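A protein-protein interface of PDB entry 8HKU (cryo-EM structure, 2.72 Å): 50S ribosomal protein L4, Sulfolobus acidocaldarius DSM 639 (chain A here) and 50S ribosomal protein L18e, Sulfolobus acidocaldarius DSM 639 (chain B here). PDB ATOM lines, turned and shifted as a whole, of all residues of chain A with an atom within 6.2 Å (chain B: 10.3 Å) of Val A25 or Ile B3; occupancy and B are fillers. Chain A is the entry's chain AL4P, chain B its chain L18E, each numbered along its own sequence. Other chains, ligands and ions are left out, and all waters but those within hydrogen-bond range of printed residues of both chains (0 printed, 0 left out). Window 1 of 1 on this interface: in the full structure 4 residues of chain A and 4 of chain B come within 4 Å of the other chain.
The backbone carbonyl oxygen (O) of Thr B1 lies close to the side-chain carboxylate (OD1) of Asp A28, at 3.2 Å.
OD1 of Asn B2 lies within hydrogen-bond range of N of Met B4, at 3.1 Å.
O of Pro A24 sits at hydrogen-bond distance from OG of Ser A114, at 3.3 Å.
The guanidinium group (NH2) of Arg A26 lies within salt-bridge range of the side-chain carboxylate (OD2) of Asp A28.
OG of Ser A114 sits at hydrogen-bond distance from N of Arg A26.
Pro A24 touches Met B4 (CB to CE, 3.6 Å).
Ile B3 touches Val A25.
NH1 of Arg A26 touches ND2 of Asn B2, at 3.6 Å.
Val A25 touches just one residue of chain B: Ile B3.
Of the printed residues of chain B, Asp A28 touches Thr B1.
Of the printed residues of chain A, Asn B2 touches Arg A26.
Of the printed residues of chain A, Ile B3 touches Val A25 (3.9 Å).
Printed residues of chain A within 4 Å of Met B4: Pro A24.
The nearest printed residue of chain B that does not touch Asp A28 is Asn B2 (4.002 Å).
Printed residues of chain A that touch a printed residue of chain B: Pro A24, Val A25, Arg A26 and Asp A28.
Hydrophobic or aromatic side chains of chain A that line the printed part of chain B: Pro A24.
Along chain A the printed residues that touch a printed residue of chain B span positions 24 to 28.
Among the printed residues, 4 pairs touch across the chains.
Among the printed residues, no Asp or Glu carboxylate lies within 4 Å of a Lys or Arg side-chain nitrogen of the other chain.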
ATOM      1  N   TYR A  23      22.189  25.283  -5.586  1.00  0.00           N
ATOM      2  CA  TYR A  23      21.517  24.114  -5.048  1.00  0.00           C
ATOM      3  C   TYR A  23      22.528  23.204  -4.354  1.00  0.00           C
ATOM      4  O   TYR A  23      23.680  23.119  -4.781  1.00  0.00           O
ATOM      5  CB  TYR A  23      20.811  23.359  -6.171  1.00  0.00           C
ATOM      6  CG  TYR A  23      19.786  22.361  -5.705  1.00  0.00           C
ATOM      7  CD1 TYR A  23      18.608  22.775  -5.114  1.00  0.00           C
ATOM      8  CD2 TYR A  23      19.994  21.007  -5.862  1.00  0.00           C
ATOM      9  CE1 TYR A  23      17.677  21.868  -4.687  1.00  0.00           C
ATOM     10  CE2 TYR A  23      19.068  20.094  -5.440  1.00  0.00           C
ATOM     11  CZ  TYR A  23      17.912  20.529  -4.852  1.00  0.00           C
ATOM     12  OH  TYR A  23      16.983  19.614  -4.427  1.00  0.00           O
ATOM     13  N   PRO A  24      22.139  22.529  -3.275  1.00  0.00           N
ATOM     14  CA  PRO A  24      23.054  21.578  -2.638  1.00  0.00           C
ATOM     15  C   PRO A  24      23.376  20.405  -3.549  1.00  0.00           C
ATOM     16  O   PRO A  24      22.574  20.007  -4.393  1.00  0.00           O
ATOM     17  CB  PRO A  24      22.281  21.123  -1.396  1.00  0.00           C
ATOM     18  CG  PRO A  24      20.865  21.434  -1.695  1.00  0.00           C
ATOM     19  CD  PRO A  24      20.902  22.686  -2.498  1.00  0.00           C
ATOM     20  N   VAL A  25      24.568  19.852  -3.368  1.00  0.00           N
ATOM     21  CA  VAL A  25      25.014  18.706  -4.154  1.00  0.00           C
ATOM     22  C   VAL A  25      24.506  17.433  -3.494  1.00  0.00           C
ATOM     23  O   VAL A  25      24.805  17.166  -2.327  1.00  0.00           O
ATOM     24  CB  VAL A  25      26.540  18.684  -4.284  1.00  0.00           C
ATOM     25  CG1 VAL A  25      26.978  17.426  -4.967  1.00  0.00           C
ATOM     26  CG2 VAL A  25      27.017  19.886  -5.046  1.00  0.00           C
ATOM     27  N   ARG A  26      23.757  16.635  -4.239  1.00  0.00           N
ATOM     28  CA  ARG A  26      23.106  15.451  -3.694  1.00  0.00           C
ATOM     29  C   ARG A  26      23.633  14.223  -4.418  1.00  0.00           C
ATOM     30  O   ARG A  26      23.142  13.872  -5.490  1.00  0.00           O
ATOM     31  CB  ARG A  26      21.599  15.571  -3.823  1.00  0.00           C
ATOM     32  CG  ARG A  26      21.005  16.640  -2.940  1.00  0.00           C
ATOM     33  CD  ARG A  26      19.522  16.590  -3.022  1.00  0.00           C
ATOM     34  NE  ARG A  26      19.060  15.214  -2.954  1.00  0.00           N
ATOM     35  CZ  ARG A  26      17.799  14.861  -2.772  1.00  0.00           C
ATOM     36  NH1 ARG A  26      16.848  15.762  -2.619  1.00  0.00           N
ATOM     37  NH2 ARG A  26      17.485  13.572  -2.746  1.00  0.00           N
ATOM     38  N   LYS A  27      24.618  13.559  -3.815  1.00  0.00           N
ATOM     39  CA  LYS A  27      25.273  12.431  -4.468  1.00  0.00           C
ATOM     40  C   LYS A  27      24.329  11.258  -4.669  1.00  0.00           C
ATOM     41  O   LYS A  27      24.519  10.465  -5.592  1.00  0.00           O
ATOM     42  CB  LYS A  27      26.486  11.998  -3.654  1.00  0.00           C
ATOM     43  CG  LYS A  27      27.540  13.064  -3.541  1.00  0.00           C
ATOM     44  CD  LYS A  27      28.791  12.527  -2.895  1.00  0.00           C
ATOM     45  CE  LYS A  27      29.869  13.587  -2.855  1.00  0.00           C
ATOM     46  NZ  LYS A  27      31.041  13.150  -2.057  1.00  0.00           N
ATOM     47  N   ASP A  28      23.321  11.116  -3.815  1.00  0.00           N
ATOM     48  CA  ASP A  28      22.360  10.033  -3.982  1.00  0.00           C
ATOM     49  C   ASP A  28      21.458  10.261  -5.184  1.00  0.00           C
ATOM     50  O   ASP A  28      21.024   9.301  -5.822  1.00  0.00           O
ATOM     51  CB  ASP A  28      21.515   9.893  -2.722  1.00  0.00           C
ATOM     52  CG  ASP A  28      20.847  11.196  -2.317  1.00  0.00           C
ATOM     53  OD1 ASP A  28      21.492  12.013  -1.627  1.00  0.00           O
ATOM     54  OD2 ASP A  28      19.672  11.400  -2.679  1.00  0.00           O
ATOM     55  N   ILE A  30      22.331  12.166  -7.920  1.00  0.00           N
ATOM     56  CA  ILE A  30      23.158  12.096  -9.117  1.00  0.00           C
ATOM     57  C   ILE A  30      23.431  10.649  -9.500  1.00  0.00           C
ATOM     58  O   ILE A  30      23.492  10.308 -10.684  1.00  0.00           O
ATOM     59  CB  ILE A  30      24.456  12.881  -8.887  1.00  0.00           C
ATOM     60  CG1 ILE A  30      24.129  14.349  -8.656  1.00  0.00           C
ATOM     61  CG2 ILE A  30      25.398  12.717 -10.053  1.00  0.00           C
ATOM     62  CD1 ILE A  30      25.268  15.148  -8.143  1.00  0.00           C
ATOM     63  N   SER A 114      21.563  19.547  -9.835  1.00  0.00           N
ATOM     64  CA  SER A 114      22.460  19.263  -8.724  1.00  0.00           C
ATOM     65  C   SER A 114      23.888  19.043  -9.194  1.00  0.00           C
ATOM     66  O   SER A 114      24.835  19.390  -8.484  1.00  0.00           O
ATOM     67  CB  SER A 114      21.955  18.046  -7.958  1.00  0.00           C
ATOM     68  OG  SER A 114      22.766  17.796  -6.837  1.00  0.00           O
ATOM     69  N   ALA A 117      25.602  22.448 -10.120  1.00  0.00           N
ATOM     70  CA  ALA A 117      26.088  23.169  -8.954  1.00  0.00           C
ATOM     71  C   ALA A 117      27.398  22.602  -8.435  1.00  0.00           C
ATOM     72  O   ALA A 117      28.216  23.349  -7.893  1.00  0.00           O
ATOM     73  CB  ALA A 117      25.039  23.141  -7.847  1.00  0.00           C
ATOM     74  N   ALA A 118      27.618  21.298  -8.591  1.00  0.00           N
ATOM     75  CA  ALA A 118      28.861  20.690  -8.138  1.00  0.00           C
ATOM     76  C   ALA A 118      30.062  21.159  -8.939  1.00  0.00           C
ATOM     77  O   ALA A 118      31.191  21.022  -8.466  1.00  0.00           O
ATOM     78  CB  ALA A 118      28.762  19.171  -8.195  1.00  0.00           C
ATOM     79  N   THR A 119      29.856  21.695 -10.136  1.00  0.00           N
ATOM     80  CA  THR A 119      30.950  22.255 -10.910  1.00  0.00           C
ATOM     81  C   THR A 119      31.234  23.705 -10.563  1.00  0.00           C
ATOM     82  O   THR A 119      32.199  24.269 -11.080  1.00  0.00           O
ATOM     83  CB  THR A 119      30.662  22.151 -12.406  1.00  0.00           C
ATOM     84  OG1 THR A 119      29.703  23.143 -12.778  1.00  0.00           O
ATOM     85  CG2 THR A 119      30.113  20.789 -12.733  1.00  0.00           C
ATOM     86  N   ASP A 121      31.453  24.465  -7.222  1.00  0.00           N
ATOM     87  CA  ASP A 121      32.001  24.342  -5.882  1.00  0.00           C
ATOM     88  C   ASP A 121      33.451  23.903  -5.979  1.00  0.00           C
ATOM     89  O   ASP A 121      33.713  22.765  -6.390  1.00  0.00           O
ATOM     90  CB  ASP A 121      31.198  23.336  -5.064  1.00  0.00           C
ATOM     91  CG  ASP A 121      31.366  23.533  -3.574  1.00  0.00           C
ATOM     92  OD1 ASP A 121      32.263  24.302  -3.170  1.00  0.00           O
ATOM     93  OD2 ASP A 121      30.603  22.920  -2.802  1.00  0.00           O
ATOM     94  N   PHE A 124      34.449  20.323  -4.502  1.00  0.00           N
ATOM     95  CA  PHE A 124      34.116  19.101  -5.222  1.00  0.00           C
ATOM     96  C   PHE A 124      34.998  18.907  -6.445  1.00  0.00           C
ATOM     97  O   PHE A 124      35.269  17.770  -6.837  1.00  0.00           O
ATOM     98  CB  PHE A 124      32.649  19.118  -5.632  1.00  0.00           C
ATOM     99  CG  PHE A 124      31.716  18.707  -4.541  1.00  0.00           C
ATOM    100  CD1 PHE A 124      31.401  17.380  -4.349  1.00  0.00           C
ATOM    101  CD2 PHE A 124      31.154  19.648  -3.703  1.00  0.00           C
ATOM    102  CE1 PHE A 124      30.546  17.003  -3.342  1.00  0.00           C
ATOM    103  CE2 PHE A 124      30.299  19.275  -2.699  1.00  0.00           C
ATOM    104  CZ  PHE A 124      29.994  17.952  -2.519  1.00  0.00           C
ATOM    105  N   PRO A 234      30.371  13.595  -8.840  1.00  0.00           N
ATOM    106  CA  PRO A 234      30.164  14.964  -9.309  1.00  0.00           C
ATOM    107  C   PRO A 234      31.420  15.804  -9.187  1.00  0.00           C
ATOM    108  O   PRO A 234      32.320  15.520  -8.400  1.00  0.00           O
ATOM    109  CB  PRO A 234      29.067  15.493  -8.381  1.00  0.00           C
ATOM    110  CG  PRO A 234      28.626  14.323  -7.564  1.00  0.00           C
ATOM    111  CD  PRO A 234      29.735  13.364  -7.541  1.00  0.00           C
ATOM    112  N   THR B   1      18.650   9.064   3.344  1.00  0.00           N
ATOM    113  CA  THR B   1      19.526   9.024   2.179  1.00  0.00           C
ATOM    114  C   THR B   1      19.901  10.425   1.716  1.00  0.00           C
ATOM    115  O   THR B   1      20.988  10.642   1.197  1.00  0.00           O
ATOM    116  CB  THR B   1      18.881   8.242   1.032  1.00  0.00           C
ATOM    117  OG1 THR B   1      18.682   6.885   1.434  1.00  0.00           O
ATOM    118  CG2 THR B   1      19.756   8.236  -0.164  1.00  0.00           C
ATOM    119  N   ASN B   2      19.004  11.378   1.930  1.00  0.00           N
ATOM    120  CA  ASN B   2      19.298  12.772   1.633  1.00  0.00           C
ATOM    121  C   ASN B   2      20.366  13.310   2.583  1.00  0.00           C
ATOM    122  O   ASN B   2      20.300  13.106   3.794  1.00  0.00           O
ATOM    123  CB  ASN B   2      18.017  13.593   1.748  1.00  0.00           C
ATOM    124  CG  ASN B   2      18.141  14.967   1.148  1.00  0.00           C
ATOM    125  OD1 ASN B   2      19.230  15.430   0.842  1.00  0.00           O
ATOM    126  ND2 ASN B   2      17.012  15.631   0.974  1.00  0.00           N
ATOM    127  N   ILE B   3      21.347  14.019   2.026  1.00  0.00           N
ATOM    128  CA  ILE B   3      22.416  14.596   2.837  1.00  0.00           C
ATOM    129  C   ILE B   3      21.895  15.721   3.720  1.00  0.00           C
ATOM    130  O   ILE B   3      22.347  15.887   4.855  1.00  0.00           O
ATOM    131  CB  ILE B   3      23.579  15.064   1.936  1.00  0.00           C
ATOM    132  CG1 ILE B   3      24.827  15.401   2.757  1.00  0.00           C
ATOM    133  CG2 ILE B   3      23.176  16.235   1.048  1.00  0.00           C
ATOM    134  CD1 ILE B   3      25.123  14.461   3.860  1.00  0.00           C
ATOM    135  N   MET B   4      20.955  16.518   3.221  1.00  0.00           N
ATOM    136  CA  MET B   4      20.507  17.676   3.980  1.00  0.00           C
ATOM    137  C   MET B   4      19.437  17.317   4.996  1.00  0.00           C
ATOM    138  O   MET B   4      19.289  18.016   6.001  1.00  0.00           O
ATOM    139  CB  MET B   4      19.999  18.757   3.032  1.00  0.00           C
ATOM    140  CG  MET B   4      21.085  19.314   2.152  1.00  0.00           C
ATOM    141  SD  MET B   4      22.342  20.145   3.135  1.00  0.00           S
ATOM    142  CE  MET B   4      23.591  20.484   1.903  1.00  0.00           C
ATOM    143  N   LEU B   5      18.678  16.255   4.754  1.00  0.00           N
ATOM    144  CA  LEU B   5      17.730  15.799   5.756  1.00  0.00           C
ATOM    145  C   LEU B   5      18.448  15.197   6.949  1.00  0.00           C
ATOM    146  O   LEU B   5      17.971  15.307   8.079  1.00  0.00           O
ATOM    147  CB  LEU B   5      16.764  14.793   5.141  1.00  0.00           C
ATOM    148  CG  LEU B   5      15.659  14.262   6.046  1.00  0.00           C
ATOM    149  CD1 LEU B   5      14.850  15.397   6.609  1.00  0.00           C
ATOM    150  CD2 LEU B   5      14.770  13.311   5.286  1.00  0.00           C
ATOM    151  N   ARG B   6      19.598  14.570   6.720  1.00  0.00           N
ATOM    152  CA  ARG B   6      20.360  13.980   7.813  1.00  0.00           C
ATOM    153  C   ARG B   6      21.016  15.045   8.675  1.00  0.00           C
ATOM    154  O   ARG B   6      21.054  14.919   9.901  1.00  0.00           O
ATOM    155  CB  ARG B   6      21.403  13.028   7.250  1.00  0.00           C
ATOM    156  CG  ARG B   6      20.815  11.780   6.665  1.00  0.00           C
ATOM    157  CD  ARG B   6      21.895  10.856   6.176  1.00  0.00           C
ATOM    158  NE  ARG B   6      21.476   9.467   6.266  1.00  0.00           N
ATOM    159  CZ  ARG B   6      22.088   8.558   7.008  1.00  0.00           C
ATOM    160  NH1 ARG B   6      23.156   8.861   7.724  1.00  0.00           N
ATOM    161  NH2 ARG B   6      21.611   7.319   7.041  1.00  0.00           N
ATOM    162  N   LYS B   7      21.561  16.088   8.057  1.00  0.00           N
ATOM    163  CA  LYS B   7      22.156  17.168   8.828  1.00  0.00           C
ATOM    164  C   LYS B   7      21.115  18.018   9.538  1.00  0.00           C
ATOM    165  O   LYS B   7      21.448  18.696  10.512  1.00  0.00           O
ATOM    166  CB  LYS B   7      23.007  18.049   7.923  1.00  0.00           C
ATOM    167  CG  LYS B   7      24.317  17.433   7.504  1.00  0.00           C
ATOM    168  CD  LYS B   7      25.168  18.460   6.799  1.00  0.00           C
ATOM    169  CE  LYS B   7      26.593  17.990   6.647  1.00  0.00           C
ATOM    170  NZ  LYS B   7      27.396  18.960   5.858  1.00  0.00           N
ATOM    171  N   LEU B   8      19.873  18.021   9.060  1.00  0.00           N
ATOM    172  CA  LEU B   8      18.816  18.742   9.758  1.00  0.00           C
ATOM    173  C   LEU B   8      18.353  17.983  10.991  1.00  0.00           C
ATOM    174  O   LEU B   8      18.079  18.589  12.029  1.00  0.00           O
ATOM    175  CB  LEU B   8      17.644  18.997   8.816  1.00  0.00           C
ATOM    176  CG  LEU B   8      16.397  19.598   9.457  1.00  0.00           C
ATOM    177  CD1 LEU B   8      16.618  21.055   9.775  1.00  0.00           C
ATOM    178  CD2 LEU B   8      15.206  19.430   8.561  1.00  0.00           C
ATOM    179  N   ILE B   9      18.256  16.657  10.895  1.00  0.00           N
ATOM    180  CA  ILE B   9      17.838  15.858  12.041  1.00  0.00           C
ATOM    181  C   ILE B   9      18.853  15.950  13.169  1.00  0.00           C
ATOM    182  O   ILE B   9      18.486  15.992  14.347  1.00  0.00           O
ATOM    183  CB  ILE B   9      17.599  14.401  11.621  1.00  0.00           C
ATOM    184  CG1 ILE B   9      16.458  14.311  10.616  1.00  0.00           C
ATOM    185  CG2 ILE B   9      17.321  13.545  12.822  1.00  0.00           C
ATOM    186  CD1 ILE B   9      16.047  12.906  10.311  1.00  0.00           C
ATOM    187  N   THR B  10      20.143  15.980  12.840  1.00  0.00           N
ATOM    188  CA  THR B  10      21.152  15.999  13.888  1.00  0.00           C
ATOM    189  C   THR B  10      21.194  17.326  14.630  1.00  0.00           C
ATOM    190  O   THR B  10      21.657  17.361  15.771  1.00  0.00           O
ATOM    191  CB  THR B  10      22.534  15.685  13.314  1.00  0.00           C
ATOM    192  OG1 THR B  10      23.465  15.519  14.385  1.00  0.00           O
ATOM    193  CG2 THR B  10      23.021  16.812  12.446  1.00  0.00           C
ATOM    194  N   SER B  11      20.722  18.409  14.023  1.00  0.00           N
ATOM    195  CA  SER B  11      20.739  19.701  14.691  1.00  0.00           C
ATOM    196  C   SER B  11      19.444  19.992  15.426  1.00  0.00           C
ATOM    197  O   SER B  11      19.443  20.795  16.362  1.00  0.00           O
ATOM    198  CB  SER B  11      21.014  20.816  13.687  1.00  0.00           C
ATOM    199  OG  SER B  11      19.952  20.923  12.771  1.00  0.00           O
ATOM    200  N   LEU B  73       8.902  21.159   6.365  1.00  0.00           N
ATOM    201  CA  LEU B  73      10.048  20.623   5.643  1.00  0.00           C
ATOM    202  C   LEU B  73      10.049  21.082   4.193  1.00  0.00           C
ATOM    203  O   LEU B  73      11.077  21.517   3.669  1.00  0.00           O
ATOM    204  CB  LEU B  73      10.041  19.100   5.722  1.00  0.00           C
ATOM    205  CG  LEU B  73      11.209  18.399   5.042  1.00  0.00           C
ATOM    206  CD1 LEU B  73      12.489  18.702   5.779  1.00  0.00           C
ATOM    207  CD2 LEU B  73      10.960  16.911   4.988  1.00  0.00           C
ATOM    208  N   TYR B  94      15.076  24.743   8.788  1.00  0.00           N
ATOM    209  CA  TYR B  94      16.423  25.239   9.033  1.00  0.00           C
ATOM    210  C   TYR B  94      16.399  26.672   9.545  1.00  0.00           C
ATOM    211  O   TYR B  94      17.116  27.012  10.490  1.00  0.00           O
ATOM    212  CB  TYR B  94      17.238  25.129   7.747  1.00  0.00           C
ATOM    213  CG  TYR B  94      18.716  25.370   7.900  1.00  0.00           C
ATOM    214  CD1 TYR B  94      19.220  26.649   8.078  1.00  0.00           C
ATOM    215  CD2 TYR B  94      19.611  24.316   7.858  1.00  0.00           C
ATOM    216  CE1 TYR B  94      20.572  26.870   8.212  1.00  0.00           C
ATOM    217  CE2 TYR B  94      20.964  24.527   7.991  1.00  0.00           C
ATOM    218  CZ  TYR B  94      21.440  25.806   8.168  1.00  0.00           C
ATOM    219  OH  TYR B  94      22.791  26.019   8.302  1.00  0.00           O
